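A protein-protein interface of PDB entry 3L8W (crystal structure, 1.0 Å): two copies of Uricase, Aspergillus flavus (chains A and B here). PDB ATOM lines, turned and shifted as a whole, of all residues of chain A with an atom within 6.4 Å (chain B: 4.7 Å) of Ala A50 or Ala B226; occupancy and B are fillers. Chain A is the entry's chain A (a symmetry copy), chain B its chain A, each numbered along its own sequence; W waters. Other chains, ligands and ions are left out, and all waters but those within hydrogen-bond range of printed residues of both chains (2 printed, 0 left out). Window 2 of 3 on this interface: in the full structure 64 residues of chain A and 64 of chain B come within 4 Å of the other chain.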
ATOM      1  N   THR A  45      24.109  24.318  14.747  1.00  0.00           N
ATOM      2  CA  THR A  45      23.679  25.713  14.817  1.00  0.00           C
ATOM      3  C   THR A  45      22.190  25.903  14.670  1.00  0.00           C
ATOM      4  O   THR A  45      21.682  26.976  15.014  1.00  0.00           O
ATOM      5  CB  THR A  45      24.410  26.565  13.769  1.00  0.00           C
ATOM      6  OG1 THR A  45      24.165  26.034  12.452  1.00  0.00           O
ATOM      7  CG2 THR A  45      25.912  26.562  14.058  1.00  0.00           C
ATOM      8  N   SER A  46      21.452  24.886  14.217  1.00  0.00           N
ATOM      9  CA  SER A  46      19.977  24.988  14.234  1.00  0.00           C
ATOM     10  C   SER A  46      19.480  25.024  15.670  1.00  0.00           C
ATOM     11  O   SER A  46      18.449  25.627  15.984  1.00  0.00           O
ATOM     12  CB  SER A  46      19.323  23.880  13.410  1.00  0.00           C
ATOM     13  OG  SER A  46      19.455  22.587  13.959  1.00  0.00           O
ATOM     14  N   TYR A  47      20.202  24.346  16.557  1.00  0.00           N
ATOM     15  CA  TYR A  47      19.883  24.294  17.979  1.00  0.00           C
ATOM     16  C   TYR A  47      20.406  25.502  18.730  1.00  0.00           C
ATOM     17  O   TYR A  47      19.736  26.061  19.600  1.00  0.00           O
ATOM     18  CB  TYR A  47      20.449  22.998  18.569  1.00  0.00           C
ATOM     19  CG  TYR A  47      19.895  21.693  17.993  1.00  0.00           C
ATOM     20  CD1 TYR A  47      20.424  21.128  16.844  1.00  0.00           C
ATOM     21  CD2 TYR A  47      18.834  21.016  18.594  1.00  0.00           C
ATOM     22  CE1 TYR A  47      19.937  19.939  16.308  1.00  0.00           C
ATOM     23  CE2 TYR A  47      18.354  19.808  18.081  1.00  0.00           C
ATOM     24  CZ  TYR A  47      18.892  19.250  16.945  1.00  0.00           C
ATOM     25  OH  TYR A  47      18.421  18.082  16.404  1.00  0.00           O
ATOM     26  N   THR A  48      21.653  25.910  18.442  1.00  0.00           N
ATOM     27  CA  THR A  48      22.285  26.920  19.305  1.00  0.00           C
ATOM     28  C   THR A  48      22.125  28.338  18.805  1.00  0.00           C
ATOM     29  O   THR A  48      22.272  29.258  19.660  1.00  0.00           O
ATOM     30  CB  THR A  48      23.802  26.640  19.426  1.00  0.00           C
ATOM     31  OG1 THR A  48      24.349  26.687  18.103  1.00  0.00           O
ATOM     32  CG2 THR A  48      24.099  25.256  19.953  1.00  0.00           C
ATOM     33  N   LYS A  49      21.846  28.557  17.529  1.00  0.00           N
ATOM     34  CA  LYS A  49      21.883  29.929  16.939  1.00  0.00           C
ATOM     35  C   LYS A  49      20.640  30.187  16.098  1.00  0.00           C
ATOM     36  O   LYS A  49      20.612  31.192  15.367  1.00  0.00           O
ATOM     37  CB  LYS A  49      23.118  30.100  16.076  1.00  0.00           C
ATOM     38  CG  LYS A  49      24.490  30.067  16.682  1.00  0.00           C
ATOM     39  CD  LYS A  49      24.674  30.927  17.909  1.00  0.00           C
ATOM     40  CE  LYS A  49      26.085  30.693  18.469  1.00  0.00           C
ATOM     41  NZ  LYS A  49      26.283  31.632  19.627  1.00  0.00           N
ATOM     42  N   ALA A  50      19.610  29.322  16.192  1.00  0.00           N
ATOM     43  CA  ALA A  50      18.396  29.554  15.393  1.00  0.00           C
ATOM     44  C   ALA A  50      18.735  29.605  13.907  1.00  0.00           C
ATOM     45  O   ALA A  50      18.068  30.318  13.145  1.00  0.00           O
ATOM     46  CB  ALA A  50      17.611  30.789  15.824  1.00  0.00           C
ATOM     47  N   ASP A  51      19.710  28.824  13.465  1.00  0.00           N
ATOM     48  CA  ASP A  51      20.129  28.800  12.057  1.00  0.00           C
ATOM     49  C   ASP A  51      19.458  27.646  11.331  1.00  0.00           C
ATOM     50  O   ASP A  51      19.943  26.506  11.333  1.00  0.00           O
ATOM     51  CB  ASP A  51      21.642  28.671  11.982  1.00  0.00           C
ATOM     52  CG  ASP A  51      22.194  28.350  10.620  1.00  0.00           C
ATOM     53  OD1 ASP A  51      21.513  28.646   9.599  1.00  0.00           O
ATOM     54  OD2 ASP A  51      23.341  27.828  10.524  1.00  0.00           O
ATOM     55  N   ASN A  52      18.311  27.921  10.677  1.00  0.00           N
ATOM     56  CA  ASN A  52      17.591  26.864  10.001  1.00  0.00           C
ATOM     57  C   ASN A  52      18.162  26.510   8.634  1.00  0.00           C
ATOM     58  O   ASN A  52      17.721  25.546   7.984  1.00  0.00           O
ATOM     59  CB  ASN A  52      16.092  27.215   9.908  1.00  0.00           C
ATOM     60  CG  ASN A  52      15.411  27.191  11.250  1.00  0.00           C
ATOM     61  OD1 ASN A  52      15.822  26.434  12.138  1.00  0.00           O
ATOM     62  ND2 ASN A  52      14.348  27.967  11.401  1.00  0.00           N
ATOM     63  N   SER A  53      19.197  27.251   8.163  1.00  0.00           N
ATOM     64  CA  SER A  53      19.766  26.943   6.834  1.00  0.00           C
ATOM     65  C   SER A  53      20.324  25.515   6.697  1.00  0.00           C
ATOM     66  O   SER A  53      20.439  24.983   5.566  1.00  0.00           O
ATOM     67  CB  SER A  53      20.834  27.992   6.493  1.00  0.00           C
ATOM     68  OG  SER A  53      22.017  27.742   7.251  1.00  0.00           O
ATOM     69  N   GLN B 159       7.412  29.771  14.895  1.00  0.00           N
ATOM     70  CA  GLN B 159       7.756  30.087  13.534  1.00  0.00           C
ATOM     71  C   GLN B 159       8.623  28.964  12.937  1.00  0.00           C
ATOM     72  O   GLN B 159       9.270  28.208  13.650  1.00  0.00           O
ATOM     73  CB  GLN B 159       8.547  31.408  13.489  1.00  0.00           C
ATOM     74  CG  GLN B 159       7.845  32.540  14.253  1.00  0.00           C
ATOM     75  CD  GLN B 159       8.595  33.841  14.147  1.00  0.00           C
ATOM     76  OE1 GLN B 159       9.177  34.186  13.132  1.00  0.00           O
ATOM     77  NE2 GLN B 159       8.578  34.583  15.240  1.00  0.00           N
ATOM     78  N   PHE B 160       8.694  28.885  11.604  1.00  0.00           N
ATOM     79  CA  PHE B 160       9.653  27.978  10.949  1.00  0.00           C
ATOM     80  C   PHE B 160       9.868  28.455   9.520  1.00  0.00           C
ATOM     81  O   PHE B 160       9.077  28.233   8.603  1.00  0.00           O
ATOM     82  CB  PHE B 160       9.207  26.501  10.958  1.00  0.00           C
ATOM     83  CG  PHE B 160      10.321  25.573  10.541  1.00  0.00           C
ATOM     84  CD1 PHE B 160      11.483  25.554  11.322  1.00  0.00           C
ATOM     85  CD2 PHE B 160      10.203  24.747   9.455  1.00  0.00           C
ATOM     86  CE1 PHE B 160      12.491  24.696  10.963  1.00  0.00           C
ATOM     87  CE2 PHE B 160      11.228  23.886   9.052  1.00  0.00           C
ATOM     88  CZ  PHE B 160      12.396  23.872   9.843  1.00  0.00           C
ATOM     89  N   ASN B 224       9.484  32.721  21.740  1.00  0.00           N
ATOM     90  CA  ASN B 224       8.913  32.922  20.404  1.00  0.00           C
ATOM     91  C   ASN B 224       9.785  32.089  19.488  1.00  0.00           C
ATOM     92  O   ASN B 224      10.874  32.472  19.076  1.00  0.00           O
ATOM     93  CB  ASN B 224       8.843  34.414  20.046  1.00  0.00           C
ATOM     94  CG  ASN B 224       8.008  34.622  18.796  1.00  0.00           C
ATOM     95  OD1 ASN B 224       7.711  33.701  18.043  1.00  0.00           O
ATOM     96  ND2 ASN B 224       7.644  35.891  18.562  1.00  0.00           N
ATOM     97  N   SER B 225       9.336  30.880  19.271  1.00  0.00           N
ATOM     98  CA  SER B 225      10.199  29.798  18.842  1.00  0.00           C
ATOM     99  C   SER B 225      10.615  29.857  17.378  1.00  0.00           C
ATOM    100  O   SER B 225       9.773  29.921  16.477  1.00  0.00           O
ATOM    101  CB  SER B 225       9.433  28.486  19.086  1.00  0.00           C
ATOM    102  OG  SER B 225      10.098  27.374  18.483  1.00  0.00           O
ATOM    103  N   ALA B 226      11.909  29.782  17.085  1.00  0.00           N
ATOM    104  CA  ALA B 226      12.438  29.744  15.746  1.00  0.00           C
ATOM    105  C   ALA B 226      12.382  28.341  15.116  1.00  0.00           C
ATOM    106  O   ALA B 226      12.448  28.186  13.877  1.00  0.00           O
ATOM    107  CB  ALA B 226      13.882  30.223  15.754  1.00  0.00           C
ATOM    108  N   SER B 227      12.266  27.314  15.943  1.00  0.00           N
ATOM    109  CA  SER B 227      12.233  25.899  15.568  1.00  0.00           C
ATOM    110  C   SER B 227      12.138  25.102  16.850  1.00  0.00           C
ATOM    111  O   SER B 227      12.453  25.590  17.952  1.00  0.00           O
ATOM    112  CB  SER B 227      13.448  25.373  14.777  1.00  0.00           C
ATOM    113  OG  SER B 227      14.625  25.409  15.539  1.00  0.00           O
ATOM    114  N   ALA B 230      15.760  24.988  18.450  1.00  0.00           N
ATOM    115  CA  ALA B 230      16.205  26.175  19.108  1.00  0.00           C
ATOM    116  C   ALA B 230      15.553  26.236  20.473  1.00  0.00           C
ATOM    117  O   ALA B 230      16.209  26.567  21.469  1.00  0.00           O
ATOM    118  CB  ALA B 230      15.948  27.436  18.328  1.00  0.00           C
ATOM    119  N   THR B 231      14.269  25.895  20.538  1.00  0.00           N
ATOM    120  CA  THR B 231      13.572  25.994  21.808  1.00  0.00           C
ATOM    121  C   THR B 231      14.036  24.896  22.763  1.00  0.00           C
ATOM    122  O   THR B 231      14.268  25.168  23.955  1.00  0.00           O
ATOM    123  CB  THR B 231      12.051  25.892  21.583  1.00  0.00           C
ATOM    124  OG1 THR B 231      11.697  27.046  20.848  1.00  0.00           O
ATOM    125  CG2 THR B 231      11.315  25.952  22.894  1.00  0.00           C
HETATM  126  O   HOH W   1      16.503  27.032  14.661  1.00  0.00           O
HETATM  127  O   HOH W   2      18.634  27.980  21.093  1.00  0.00           O
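No position is printed for both chains.
Of the 7 pairs that touch across the chains among the printed residues, none has its exchanged pair printed and touching as well.
Ser A46 touches Ser B227 (O to OG, 3.9 Å).
Ser A46 touches Ala B230 (O to N, 3.7 Å).
Ala B230 touches Tyr A47.
Ala B226 touches Ala A50 (CB to CB, 3.8 Å).
Phe B160 touches Asn A52 (CD1 to ND2, 3.7 Å).
OD1 of Asn A52 touches CB of Ser B227, 3.7 Å away.
Of the printed residues of chain B, Ser A46 touches Ser B227 and Ala B230.
Of the printed residues of chain B, Tyr A47 touches Ala B230 (3.6 Å).
Lys A49 touches none of the printed residues of chain B.
Printed residues of chain B within 4 Å of Asn A52: Phe B160 (3.7 Å), Ala B226 (3.1 Å) and Ser B227 (3.7 Å).
Of the printed residues of chain A, Phe B160 touches Asn A52.
Of chain A, only Ala A50 and Asn A52 come within 4 Å of Ala B226.
Printed residues of chain A within 4 Å of Ser B227: Ser A46 (3.9 Å) and Asn A52 (3.7 Å).
The nearest residue of chain B that does not touch Ala A50 is Ala B230 (4.4 Å).
The nearest printed residue of chain A that does not touch Ala B226 is Asp A51 (6.4 Å).
The nearest printed residue of chain B that does not touch Ser A46 is Thr B231 (6.2 Å).
Hydrophobic or aromatic side chains of chain A within 4 Å of the printed part of chain B: Ala A50.
Along chain A the printed residues that touch a printed residue of chain B span positions 46 to 52.
Of the 8 printed residues of chain B, 4 touch a printed residue of chain A.
Printed residues of chain B that touch a printed residue of chain A: Phe B160, Ala B226, Ser B227 and Ala B230.
Among the printed residues, 7 pairs touch across the chains.
Among the printed residues, no Asp or Glu carboxylate lies within 4 Å of a Lys or Arg side-chain nitrogen of the other chain.
The backbone carbonyl oxygen (O) of Ser B227 lies within hydrogen-bond range of the side-chain hydroxyl (OG) of Ser B225 (3.0 Å).
The side-chain hydroxyl of Ser B227 is in hydrogen-bond range of the backbone NH of Ala B230 (3.2 Å).
O of Ser B227 lies within hydrogen-bond range of OG1 of Thr B231, 3.3 Å away.
N of Ala A50 is in hydrogen-bond range of O of Thr A45, at 3.3 Å.
Water W1 lies within hydrogen-bond range of OG of Ser B227, OD1 of Asn A52 and O of Ser A46.
Water W2 bridges the backbone carbonyl oxygen of Tyr A47 and the backbone carbonyl oxygen of Ala B230.
The backbone carbonyl oxygen (O) of Ala B226 sits at hydrogen-bond distance from the side-chain amide nitrogen (ND2) of Asn A52.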
